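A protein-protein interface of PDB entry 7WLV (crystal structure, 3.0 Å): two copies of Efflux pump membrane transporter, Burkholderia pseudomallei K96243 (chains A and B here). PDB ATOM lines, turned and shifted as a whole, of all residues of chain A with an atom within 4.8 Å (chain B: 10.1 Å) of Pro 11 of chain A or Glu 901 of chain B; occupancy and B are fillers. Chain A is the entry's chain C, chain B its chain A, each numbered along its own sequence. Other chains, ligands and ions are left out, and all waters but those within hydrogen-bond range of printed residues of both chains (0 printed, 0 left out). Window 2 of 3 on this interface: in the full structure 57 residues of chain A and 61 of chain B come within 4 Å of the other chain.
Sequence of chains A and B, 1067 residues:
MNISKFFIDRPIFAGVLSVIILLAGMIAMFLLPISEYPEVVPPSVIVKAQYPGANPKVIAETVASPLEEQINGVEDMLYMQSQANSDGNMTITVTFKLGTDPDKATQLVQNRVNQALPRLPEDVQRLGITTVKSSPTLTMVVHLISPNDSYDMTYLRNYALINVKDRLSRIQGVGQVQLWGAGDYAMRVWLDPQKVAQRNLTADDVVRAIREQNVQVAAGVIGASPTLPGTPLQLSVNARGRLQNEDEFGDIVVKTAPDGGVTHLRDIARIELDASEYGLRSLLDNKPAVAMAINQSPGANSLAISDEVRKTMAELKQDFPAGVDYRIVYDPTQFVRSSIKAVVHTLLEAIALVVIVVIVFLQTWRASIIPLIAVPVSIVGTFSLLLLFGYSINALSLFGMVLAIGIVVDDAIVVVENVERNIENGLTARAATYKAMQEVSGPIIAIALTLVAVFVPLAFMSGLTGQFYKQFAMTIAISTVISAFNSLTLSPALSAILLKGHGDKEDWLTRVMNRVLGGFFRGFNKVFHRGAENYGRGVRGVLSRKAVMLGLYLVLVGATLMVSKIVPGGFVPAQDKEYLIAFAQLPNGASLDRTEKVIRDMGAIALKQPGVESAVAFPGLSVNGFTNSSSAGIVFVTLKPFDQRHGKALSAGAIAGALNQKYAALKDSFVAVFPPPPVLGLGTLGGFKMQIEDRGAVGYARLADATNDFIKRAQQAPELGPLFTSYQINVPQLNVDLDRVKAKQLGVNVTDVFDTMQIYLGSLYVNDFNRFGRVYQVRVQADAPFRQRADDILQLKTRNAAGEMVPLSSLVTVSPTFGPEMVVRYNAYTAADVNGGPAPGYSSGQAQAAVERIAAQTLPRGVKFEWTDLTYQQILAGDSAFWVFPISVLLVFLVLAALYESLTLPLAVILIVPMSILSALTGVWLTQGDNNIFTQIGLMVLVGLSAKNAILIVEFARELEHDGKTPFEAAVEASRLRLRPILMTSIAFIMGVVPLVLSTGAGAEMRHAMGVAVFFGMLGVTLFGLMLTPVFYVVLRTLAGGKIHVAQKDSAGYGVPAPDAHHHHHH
The side-chain carboxylate of Glu 901 of chain B sits at hydrogen-bond distance from the backbone NH of Ile 12 of chain A (2.7 Å). The side-chain carboxylate of Glu 901 of chain B sits close to the backbone nitrogen of Pro 11 of chain A (3.2 Å).
N of Ser 902 of chain B is in hydrogen-bond range of O of Ala 897 of chain B (3.2 Å).
Arg 10 of chain A touches Glu 901 of chain B (C to OE2, 3.1 Å). CG2 of Ile 12 of chain A touches O of Ala 897 of chain B, at 3.6 Å. CG of Leu 903 of chain B touches CD1 of Ile 12 of chain A, 3.5 Å away. Phe 13 of chain A touches Ala 898 of chain B (CD2 to CB, 3.7 Å). Phe 13 of chain A touches Glu 901 of chain B (N to OE1, 3.5 Å).
Pro 11 of chain A touches one residue of chain B. Glu 901 of chain B touches just these residues of chain A: Arg 10 (3.1 Å), Pro 11 (3.2 Å), Ile 12 (2.7 Å) and Phe 13 (3.5 Å). Ile 12 of chain A touches just these residues of chain B: Ala 897, Glu 901 and Leu 903. Of the printed residues of chain A, Leu 903 of chain B touches Ile 12 (3.5 Å). Printed residues of chain A within 4 Å of Ala 898 of chain B: Phe 13. Of the printed residues of chain A, Ala 897 of chain B touches Ile 12 (3.6 Å). Of the printed residues of chain B, Phe 13 of chain A touches Ala 898 and Glu 901. Printed residues of chain B within 4 Å of Arg 10 of chain A: Glu 901. The nearest printed residue of chain A that does not touch Ala 898 of chain B is Ile 12 of chain A (4.4 Å).
Of the 11 printed residues of chain A, 4 touch a printed residue of chain B. Hydrophobic or aromatic side chains of chain A within 4 Å of the printed part of chain B: Pro 11, Ile 12 and Phe 13. Hydrophobic or aromatic side chains of chain B that line the printed part of chain A: Ala 897, Ala 898 and Leu 903. Along chain B the printed residues that touch a printed residue of chain A span positions 897 to 903.
No position is printed for both chains. Of the 7 pairs that touch across the chains among the printed residues, none has its exchanged pair printed and touching as well.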
ATOM      1  N   PHE A   7      -8.953  -3.401  10.962  1.00  0.00           N
ATOM      2  CA  PHE A   7      -8.415  -2.187  10.384  1.00  0.00           C
ATOM      3  C   PHE A   7      -7.591  -1.406  11.373  1.00  0.00           C
ATOM      4  O   PHE A   7      -6.664  -0.711  10.964  1.00  0.00           O
ATOM      5  CB  PHE A   7      -9.547  -1.315   9.825  1.00  0.00           C
ATOM      6  CG  PHE A   7     -10.256  -1.964   8.706  1.00  0.00           C
ATOM      7  CD1 PHE A   7      -9.709  -1.912   7.426  1.00  0.00           C
ATOM      8  CD2 PHE A   7     -11.418  -2.694   8.931  1.00  0.00           C
ATOM      9  CE1 PHE A   7     -10.329  -2.547   6.378  1.00  0.00           C
ATOM     10  CE2 PHE A   7     -12.052  -3.334   7.887  1.00  0.00           C
ATOM     11  CZ  PHE A   7     -11.508  -3.257   6.610  1.00  0.00           C
ATOM     12  N   ILE A   8      -7.916  -1.485  12.660  1.00  0.00           N
ATOM     13  CA  ILE A   8      -7.055  -0.868  13.660  1.00  0.00           C
ATOM     14  C   ILE A   8      -5.654  -1.445  13.521  1.00  0.00           C
ATOM     15  O   ILE A   8      -4.645  -0.729  13.594  1.00  0.00           O
ATOM     16  CB  ILE A   8      -7.626  -1.092  15.067  1.00  0.00           C
ATOM     17  CG1 ILE A   8      -9.013  -0.478  15.196  1.00  0.00           C
ATOM     18  CG2 ILE A   8      -6.745  -0.372  16.080  1.00  0.00           C
ATOM     19  CD1 ILE A   8      -9.810  -1.035  16.352  1.00  0.00           C
ATOM     20  N   ASP A   9      -5.581  -2.751  13.256  1.00  0.00           N
ATOM     21  CA  ASP A   9      -4.304  -3.425  13.096  1.00  0.00           C
ATOM     22  C   ASP A   9      -3.643  -3.169  11.744  1.00  0.00           C
ATOM     23  O   ASP A   9      -2.413  -3.239  11.646  1.00  0.00           O
ATOM     24  CB  ASP A   9      -4.514  -4.932  13.256  1.00  0.00           C
ATOM     25  CG  ASP A   9      -4.779  -5.334  14.701  1.00  0.00           C
ATOM     26  OD1 ASP A   9      -4.316  -4.582  15.605  1.00  0.00           O
ATOM     27  OD2 ASP A   9      -5.427  -6.406  14.904  1.00  0.00           O
ATOM     28  N   ARG A  10      -4.399  -2.797  10.716  1.00  0.00           N
ATOM     29  CA  ARG A  10      -3.856  -2.631   9.369  1.00  0.00           C
ATOM     30  C   ARG A  10      -4.209  -1.251   8.852  1.00  0.00           C
ATOM     31  O   ARG A  10      -5.072  -1.091   7.990  1.00  0.00           O
ATOM     32  CB  ARG A  10      -4.386  -3.727   8.462  1.00  0.00           C
ATOM     33  CG  ARG A  10      -4.132  -5.054   9.042  1.00  0.00           C
ATOM     34  CD  ARG A  10      -5.198  -5.937   8.563  1.00  0.00           C
ATOM     35  NE  ARG A  10      -5.487  -7.017   9.491  1.00  0.00           N
ATOM     36  CZ  ARG A  10      -4.970  -8.234   9.396  1.00  0.00           C
ATOM     37  NH1 ARG A  10      -4.124  -8.557   8.424  1.00  0.00           N
ATOM     38  NH2 ARG A  10      -5.340  -9.165  10.270  1.00  0.00           N
ATOM     39  N   PRO A  11      -3.554  -0.220   9.377  1.00  0.00           N
ATOM     40  CA  PRO A  11      -3.884   1.143   8.944  1.00  0.00           C
ATOM     41  C   PRO A  11      -3.688   1.362   7.456  1.00  0.00           C
ATOM     42  O   PRO A  11      -4.463   2.126   6.859  1.00  0.00           O
ATOM     43  CB  PRO A  11      -2.943   2.015   9.786  1.00  0.00           C
ATOM     44  CG  PRO A  11      -1.848   1.118  10.161  1.00  0.00           C
ATOM     45  CD  PRO A  11      -2.445  -0.243  10.337  1.00  0.00           C
ATOM     46  N   ILE A  12      -2.710   0.691   6.824  1.00  0.00           N
ATOM     47  CA  ILE A  12      -2.549   0.862   5.378  1.00  0.00           C
ATOM     48  C   ILE A  12      -3.805   0.392   4.652  1.00  0.00           C
ATOM     49  O   ILE A  12      -4.300   1.069   3.764  1.00  0.00           O
ATOM     50  CB  ILE A  12      -1.319   0.091   4.845  1.00  0.00           C
ATOM     51  CG1 ILE A  12      -0.023   0.451   5.581  1.00  0.00           C
ATOM     52  CG2 ILE A  12      -1.178   0.307   3.323  1.00  0.00           C
ATOM     53  CD1 ILE A  12       0.604   1.730   5.137  1.00  0.00           C
ATOM     54  N   PHE A  13      -4.367  -0.738   5.062  1.00  0.00           N
ATOM     55  CA  PHE A  13      -5.567  -1.265   4.425  1.00  0.00           C
ATOM     56  C   PHE A  13      -6.729  -0.284   4.543  1.00  0.00           C
ATOM     57  O   PHE A  13      -7.505  -0.089   3.589  1.00  0.00           O
ATOM     58  CB  PHE A  13      -5.916  -2.604   5.069  1.00  0.00           C
ATOM     59  CG  PHE A  13      -6.710  -3.512   4.212  1.00  0.00           C
ATOM     60  CD1 PHE A  13      -7.992  -3.181   3.813  1.00  0.00           C
ATOM     61  CD2 PHE A  13      -6.194  -4.737   3.852  1.00  0.00           C
ATOM     62  CE1 PHE A  13      -8.729  -4.057   3.031  1.00  0.00           C
ATOM     63  CE2 PHE A  13      -6.917  -5.617   3.076  1.00  0.00           C
ATOM     64  CZ  PHE A  13      -8.188  -5.286   2.664  1.00  0.00           C
ATOM     65  N   ALA A  14      -6.911   0.288   5.729  1.00  0.00           N
ATOM     66  CA  ALA A  14      -7.989   1.247   5.903  1.00  0.00           C
ATOM     67  C   ALA A  14      -7.750   2.468   5.026  1.00  0.00           C
ATOM     68  O   ALA A  14      -8.673   2.970   4.367  1.00  0.00           O
ATOM     69  CB  ALA A  14      -8.111   1.624   7.384  1.00  0.00           C
ATOM     70  N   GLY A  15      -6.504   2.942   4.993  1.00  0.00           N
ATOM     71  CA  GLY A  15      -6.160   4.035   4.103  1.00  0.00           C
ATOM     72  C   GLY A  15      -6.389   3.680   2.650  1.00  0.00           C
ATOM     73  O   GLY A  15      -6.840   4.509   1.862  1.00  0.00           O
ATOM     74  N   ALA A 493      -8.407   3.453  12.806  1.00  0.00           N
ATOM     75  CA  ALA A 493      -6.995   3.183  12.505  1.00  0.00           C
ATOM     76  C   ALA A 493      -6.156   4.452  12.602  1.00  0.00           C
ATOM     77  O   ALA A 493      -5.036   4.443  13.144  1.00  0.00           O
ATOM     78  CB  ALA A 493      -6.843   2.545  11.125  1.00  0.00           C
ATOM     79  N   ILE A 497      -3.241   5.148  15.479  1.00  0.00           N
ATOM     80  CA  ILE A 497      -1.894   5.457  15.023  1.00  0.00           C
ATOM     81  C   ILE A 497      -1.461   6.887  15.358  1.00  0.00           C
ATOM     82  O   ILE A 497      -0.268   7.211  15.259  1.00  0.00           O
ATOM     83  CB  ILE A 497      -1.880   5.149  13.509  1.00  0.00           C
ATOM     84  CG1 ILE A 497      -0.516   4.741  13.017  1.00  0.00           C
ATOM     85  CG2 ILE A 497      -2.319   6.386  12.676  1.00  0.00           C
ATOM     86  CD1 ILE A 497      -0.523   4.532  11.532  1.00  0.00           C
ATOM     87  N   MET B   1      -6.517 -16.383   6.445  1.00  0.00           N
ATOM     88  CA  MET B   1      -6.643 -15.544   5.256  1.00  0.00           C
ATOM     89  C   MET B   1      -6.712 -16.402   3.968  1.00  0.00           C
ATOM     90  O   MET B   1      -6.490 -15.882   2.864  1.00  0.00           O
ATOM     91  CB  MET B   1      -5.478 -14.524   5.193  1.00  0.00           C
ATOM     92  CG  MET B   1      -5.410 -13.545   6.406  1.00  0.00           C
ATOM     93  SD  MET B   1      -4.014 -12.371   6.520  1.00  0.00           S
ATOM     94  CE  MET B   1      -4.458 -11.179   5.246  1.00  0.00           C
ATOM     95  N   ALA B 446      -4.870 -11.469  -4.280  1.00  0.00           N
ATOM     96  CA  ALA B 446      -4.221 -10.194  -4.539  1.00  0.00           C
ATOM     97  C   ALA B 446      -3.813 -10.056  -6.008  1.00  0.00           C
ATOM     98  O   ALA B 446      -3.912  -8.966  -6.582  1.00  0.00           O
ATOM     99  CB  ALA B 446      -3.021 -10.044  -3.615  1.00  0.00           C
ATOM    100  N   PHE B 893      -0.890  -0.070  -7.128  1.00  0.00           N
ATOM    101  CA  PHE B 893      -0.142   0.289  -5.933  1.00  0.00           C
ATOM    102  C   PHE B 893      -0.968   0.054  -4.674  1.00  0.00           C
ATOM    103  O   PHE B 893      -0.473  -0.534  -3.706  1.00  0.00           O
ATOM    104  CB  PHE B 893       0.303   1.747  -6.002  1.00  0.00           C
ATOM    105  CG  PHE B 893       0.995   2.202  -4.770  1.00  0.00           C
ATOM    106  CD1 PHE B 893       2.360   1.992  -4.620  1.00  0.00           C
ATOM    107  CD2 PHE B 893       0.285   2.782  -3.730  1.00  0.00           C
ATOM    108  CE1 PHE B 893       3.024   2.378  -3.459  1.00  0.00           C
ATOM    109  CE2 PHE B 893       0.935   3.171  -2.549  1.00  0.00           C
ATOM    110  CZ  PHE B 893       2.307   2.978  -2.417  1.00  0.00           C
ATOM    111  N   LEU B 894      -2.227   0.522  -4.667  1.00  0.00           N
ATOM    112  CA  LEU B 894      -3.061   0.385  -3.477  1.00  0.00           C
ATOM    113  C   LEU B 894      -3.354  -1.073  -3.164  1.00  0.00           C
ATOM    114  O   LEU B 894      -3.278  -1.480  -2.002  1.00  0.00           O
ATOM    115  CB  LEU B 894      -4.367   1.159  -3.604  1.00  0.00           C
ATOM    116  CG  LEU B 894      -4.141   2.660  -3.814  1.00  0.00           C
ATOM    117  CD1 LEU B 894      -5.416   3.428  -4.255  1.00  0.00           C
ATOM    118  CD2 LEU B 894      -3.453   3.301  -2.650  1.00  0.00           C
ATOM    119  N   VAL B 895      -3.666  -1.891  -4.166  1.00  0.00           N
ATOM    120  CA  VAL B 895      -3.924  -3.296  -3.856  1.00  0.00           C
ATOM    121  C   VAL B 895      -2.690  -3.926  -3.233  1.00  0.00           C
ATOM    122  O   VAL B 895      -2.765  -4.577  -2.182  1.00  0.00           O
ATOM    123  CB  VAL B 895      -4.363  -4.075  -5.104  1.00  0.00           C
ATOM    124  CG1 VAL B 895      -4.228  -5.572  -4.855  1.00  0.00           C
ATOM    125  CG2 VAL B 895      -5.807  -3.758  -5.434  1.00  0.00           C
ATOM    126  N   LEU B 896      -1.524  -3.689  -3.839  1.00  0.00           N
ATOM    127  CA  LEU B 896      -0.299  -4.287  -3.312  1.00  0.00           C
ATOM    128  C   LEU B 896       0.018  -3.777  -1.903  1.00  0.00           C
ATOM    129  O   LEU B 896       0.429  -4.561  -1.038  1.00  0.00           O
ATOM    130  CB  LEU B 896       0.866  -4.051  -4.288  1.00  0.00           C
ATOM    131  CG  LEU B 896       0.764  -4.945  -5.539  1.00  0.00           C
ATOM    132  CD1 LEU B 896       2.088  -5.049  -6.269  1.00  0.00           C
ATOM    133  CD2 LEU B 896       0.209  -6.345  -5.202  1.00  0.00           C
ATOM    134  N   ALA B 897      -0.188  -2.474  -1.653  1.00  0.00           N
ATOM    135  CA  ALA B 897       0.042  -1.924  -0.321  1.00  0.00           C
ATOM    136  C   ALA B 897      -0.859  -2.587   0.698  1.00  0.00           C
ATOM    137  O   ALA B 897      -0.427  -2.901   1.809  1.00  0.00           O
ATOM    138  CB  ALA B 897      -0.182  -0.418  -0.308  1.00  0.00           C
ATOM    139  N   ALA B 898      -2.114  -2.833   0.341  1.00  0.00           N
ATOM    140  CA  ALA B 898      -2.946  -3.574   1.275  1.00  0.00           C
ATOM    141  C   ALA B 898      -2.410  -4.988   1.485  1.00  0.00           C
ATOM    142  O   ALA B 898      -2.397  -5.484   2.615  1.00  0.00           O
ATOM    143  CB  ALA B 898      -4.383  -3.601   0.804  1.00  0.00           C
ATOM    144  N   LEU B 899      -1.922  -5.636   0.427  1.00  0.00           N
ATOM    145  CA  LEU B 899      -1.421  -7.005   0.557  1.00  0.00           C
ATOM    146  C   LEU B 899      -0.225  -7.064   1.491  1.00  0.00           C
ATOM    147  O   LEU B 899      -0.112  -7.949   2.346  1.00  0.00           O
ATOM    148  CB  LEU B 899      -1.012  -7.546  -0.806  1.00  0.00           C
ATOM    149  CG  LEU B 899      -0.303  -8.901  -0.776  1.00  0.00           C
ATOM    150  CD1 LEU B 899      -1.293 -10.027  -0.551  1.00  0.00           C
ATOM    151  CD2 LEU B 899       0.439  -9.160  -2.053  1.00  0.00           C
ATOM    152  N   TYR B 900       0.703  -6.152   1.311  1.00  0.00           N
ATOM    153  CA  TYR B 900       1.918  -6.176   2.087  1.00  0.00           C
ATOM    154  C   TYR B 900       1.778  -5.410   3.383  1.00  0.00           C
ATOM    155  O   TYR B 900       2.661  -5.501   4.235  1.00  0.00           O
ATOM    156  CB  TYR B 900       3.083  -5.596   1.252  1.00  0.00           C
ATOM    157  CG  TYR B 900       3.320  -6.407  -0.020  1.00  0.00           C
ATOM    158  CD1 TYR B 900       3.261  -7.802   0.018  1.00  0.00           C
ATOM    159  CD2 TYR B 900       3.591  -5.787  -1.258  1.00  0.00           C
ATOM    160  CE1 TYR B 900       3.466  -8.565  -1.118  1.00  0.00           C
ATOM    161  CE2 TYR B 900       3.794  -6.556  -2.421  1.00  0.00           C
ATOM    162  CZ  TYR B 900       3.723  -7.954  -2.336  1.00  0.00           C
ATOM    163  OH  TYR B 900       3.920  -8.775  -3.438  1.00  0.00           O
ATOM    164  N   GLU B 901       0.681  -4.698   3.582  1.00  0.00           N
ATOM    165  CA  GLU B 901       0.623  -3.706   4.656  1.00  0.00           C
ATOM    166  C   GLU B 901       1.858  -2.808   4.617  1.00  0.00           C
ATOM    167  O   GLU B 901       2.408  -2.431   5.649  1.00  0.00           O
ATOM    168  CB  GLU B 901       0.466  -4.366   6.027  1.00  0.00           C
ATOM    169  CG  GLU B 901       0.056  -3.384   7.125  1.00  0.00           C
ATOM    170  CD  GLU B 901      -1.277  -2.688   6.847  1.00  0.00           C
ATOM    171  OE1 GLU B 901      -2.121  -3.257   6.076  1.00  0.00           O
ATOM    172  OE2 GLU B 901      -1.469  -1.578   7.426  1.00  0.00           O
ATOM    173  N   SER B 902       2.324  -2.491   3.408  1.00  0.00           N
ATOM    174  CA  SER B 902       3.496  -1.647   3.242  1.00  0.00           C
ATOM    175  C   SER B 902       3.235  -0.526   2.241  1.00  0.00           C
ATOM    176  O   SER B 902       2.571  -0.728   1.228  1.00  0.00           O
ATOM    177  CB  SER B 902       4.699  -2.459   2.765  1.00  0.00           C
ATOM    178  OG  SER B 902       5.767  -1.582   2.398  1.00  0.00           O
ATOM    179  N   LEU B 903       3.740   0.658   2.504  1.00  0.00           N
ATOM    180  CA  LEU B 903       3.660   1.638   1.441  1.00  0.00           C
ATOM    181  C   LEU B 903       4.834   1.567   0.474  1.00  0.00           C
ATOM    182  O   LEU B 903       4.866   2.336  -0.486  1.00  0.00           O
ATOM    183  CB  LEU B 903       3.579   3.061   1.981  1.00  0.00           C
ATOM    184  CG  LEU B 903       2.265   3.450   2.625  1.00  0.00           C
ATOM    185  CD1 LEU B 903       2.240   4.963   2.730  1.00  0.00           C
ATOM    186  CD2 LEU B 903       1.078   2.902   1.886  1.00  0.00           C
ATOM    187  N   THR B 904       5.845   0.762   0.739  1.00  0.00           N
ATOM    188  CA  THR B 904       7.025   0.748  -0.120  1.00  0.00           C
ATOM    189  C   THR B 904       7.275  -0.571  -0.836  1.00  0.00           C
ATOM    190  O   THR B 904       7.746  -0.550  -1.976  1.00  0.00           O
ATOM    191  CB  THR B 904       8.269   1.133   0.692  1.00  0.00           C
ATOM    192  OG1 THR B 904       8.484   0.183   1.760  1.00  0.00           O
ATOM    193  CG2 THR B 904       8.108   2.541   1.220  1.00  0.00           C
ATOM    194  N   LEU B 905       6.945  -1.706  -0.220  1.00  0.00           N
ATOM    195  CA  LEU B 905       7.126  -2.984  -0.889  1.00  0.00           C
ATOM    196  C   LEU B 905       6.420  -3.078  -2.243  1.00  0.00           C
ATOM    197  O   LEU B 905       6.932  -3.814  -3.111  1.00  0.00           O
ATOM    198  CB  LEU B 905       6.655  -4.117   0.028  1.00  0.00           C
ATOM    199  CG  LEU B 905       7.643  -5.260   0.068  1.00  0.00           C
ATOM    200  CD1 LEU B 905       9.010  -4.668   0.344  1.00  0.00           C
ATOM    201  CD2 LEU B 905       7.224  -6.233   1.148  1.00  0.00           C
ATOM    202  N   PRO B 906       5.272  -2.412  -2.493  1.00  0.00           N
ATOM    203  CA  PRO B 906       4.695  -2.473  -3.854  1.00  0.00           C
ATOM    204  C   PRO B 906       5.656  -2.076  -4.975  1.00  0.00           C
ATOM    205  O   PRO B 906       5.590  -2.715  -6.037  1.00  0.00           O
ATOM    206  CB  PRO B 906       3.486  -1.534  -3.752  1.00  0.00           C
ATOM    207  CG  PRO B 906       3.044  -1.712  -2.336  1.00  0.00           C
ATOM    208  CD  PRO B 906       4.306  -1.849  -1.530  1.00  0.00           C
ATOM    209  N   VAL B 954       7.993 -11.506  -4.134  1.00  0.00           N
ATOM    210  CA  VAL B 954       8.019 -10.586  -3.002  1.00  0.00           C
ATOM    211  C   VAL B 954       7.240 -11.167  -1.839  1.00  0.00           C
ATOM    212  O   VAL B 954       7.646 -11.033  -0.686  1.00  0.00           O
ATOM    213  CB  VAL B 954       7.482  -9.203  -3.408  1.00  0.00           C
ATOM    214  CG1 VAL B 954       7.025  -8.411  -2.170  1.00  0.00           C
ATOM    215  CG2 VAL B 954       8.537  -8.438  -4.192  1.00  0.00           C
ATOM    216  N   GLU B 955       6.111 -11.817  -2.113  1.00  0.00           N
ATOM    217  CA  GLU B 955       5.313 -12.360  -1.027  1.00  0.00           C
ATOM    218  C   GLU B 955       6.039 -13.506  -0.344  1.00  0.00           C
ATOM    219  O   GLU B 955       6.043 -13.581   0.888  1.00  0.00           O
ATOM    220  CB  GLU B 955       3.928 -12.780  -1.534  1.00  0.00           C
ATOM    221  CG  GLU B 955       2.802 -11.952  -0.935  1.00  0.00           C
ATOM    222  CD  GLU B 955       2.488 -12.371   0.504  1.00  0.00           C
ATOM    223  OE1 GLU B 955       2.371 -13.598   0.714  1.00  0.00           O
ATOM    224  OE2 GLU B 955       2.368 -11.505   1.425  1.00  0.00           O
ATOM    225  N   ARG B 958       8.859 -11.896   1.803  1.00  0.00           N
ATOM    226  CA  ARG B 958       8.235 -11.305   2.969  1.00  0.00           C
ATOM    227  C   ARG B 958       7.877 -12.386   3.993  1.00  0.00           C
ATOM    228  O   ARG B 958       8.068 -12.207   5.201  1.00  0.00           O
ATOM    229  CB  ARG B 958       7.039 -10.480   2.476  1.00  0.00           C
ATOM    230  CG  ARG B 958       6.266  -9.774   3.514  1.00  0.00           C
ATOM    231  CD  ARG B 958       5.262  -8.855   2.884  1.00  0.00           C
ATOM    232  NE  ARG B 958       4.378  -8.368   3.927  1.00  0.00           N
ATOM    233  CZ  ARG B 958       3.345  -9.071   4.363  1.00  0.00           C
ATOM    234  NH1 ARG B 958       3.083 -10.279   3.875  1.00  0.00           N
ATOM    235  NH2 ARG B 958       2.589  -8.579   5.345  1.00  0.00           N
ATOM    236  N   ARG B1037      13.369  -3.253   1.305  1.00  0.00           N
ATOM    237  CA  ARG B1037      13.197  -3.858   2.613  1.00  0.00           C
ATOM    238  C   ARG B1037      14.109  -3.234   3.664  1.00  0.00           C
ATOM    239  O   ARG B1037      13.777  -3.278   4.851  1.00  0.00           O
ATOM    240  CB  ARG B1037      13.396  -5.371   2.502  1.00  0.00           C
ATOM    241  CG  ARG B1037      12.863  -6.163   3.681  1.00  0.00           C
ATOM    242  CD  ARG B1037      11.333  -6.251   3.754  1.00  0.00           C
ATOM    243  NE  ARG B1037      10.753  -5.045   4.338  1.00  0.00           N
ATOM    244  CZ  ARG B1037      10.818  -4.725   5.622  1.00  0.00           C
ATOM    245  NH1 ARG B1037      11.452  -5.491   6.491  1.00  0.00           N
ATOM    246  NH2 ARG B1037      10.252  -3.595   6.036  1.00  0.00           N
ATOM    247  N   ALA B1040      12.428   0.312   5.748  1.00  0.00           N
ATOM    248  CA  ALA B1040      11.212   0.358   6.574  1.00  0.00           C
ATOM    249  C   ALA B1040      11.446  -0.196   7.985  1.00  0.00           C
ATOM    250  O   ALA B1040      10.724  -1.072   8.467  1.00  0.00           O
ATOM    251  CB  ALA B1040      10.057  -0.376   5.896  1.00  0.00           C
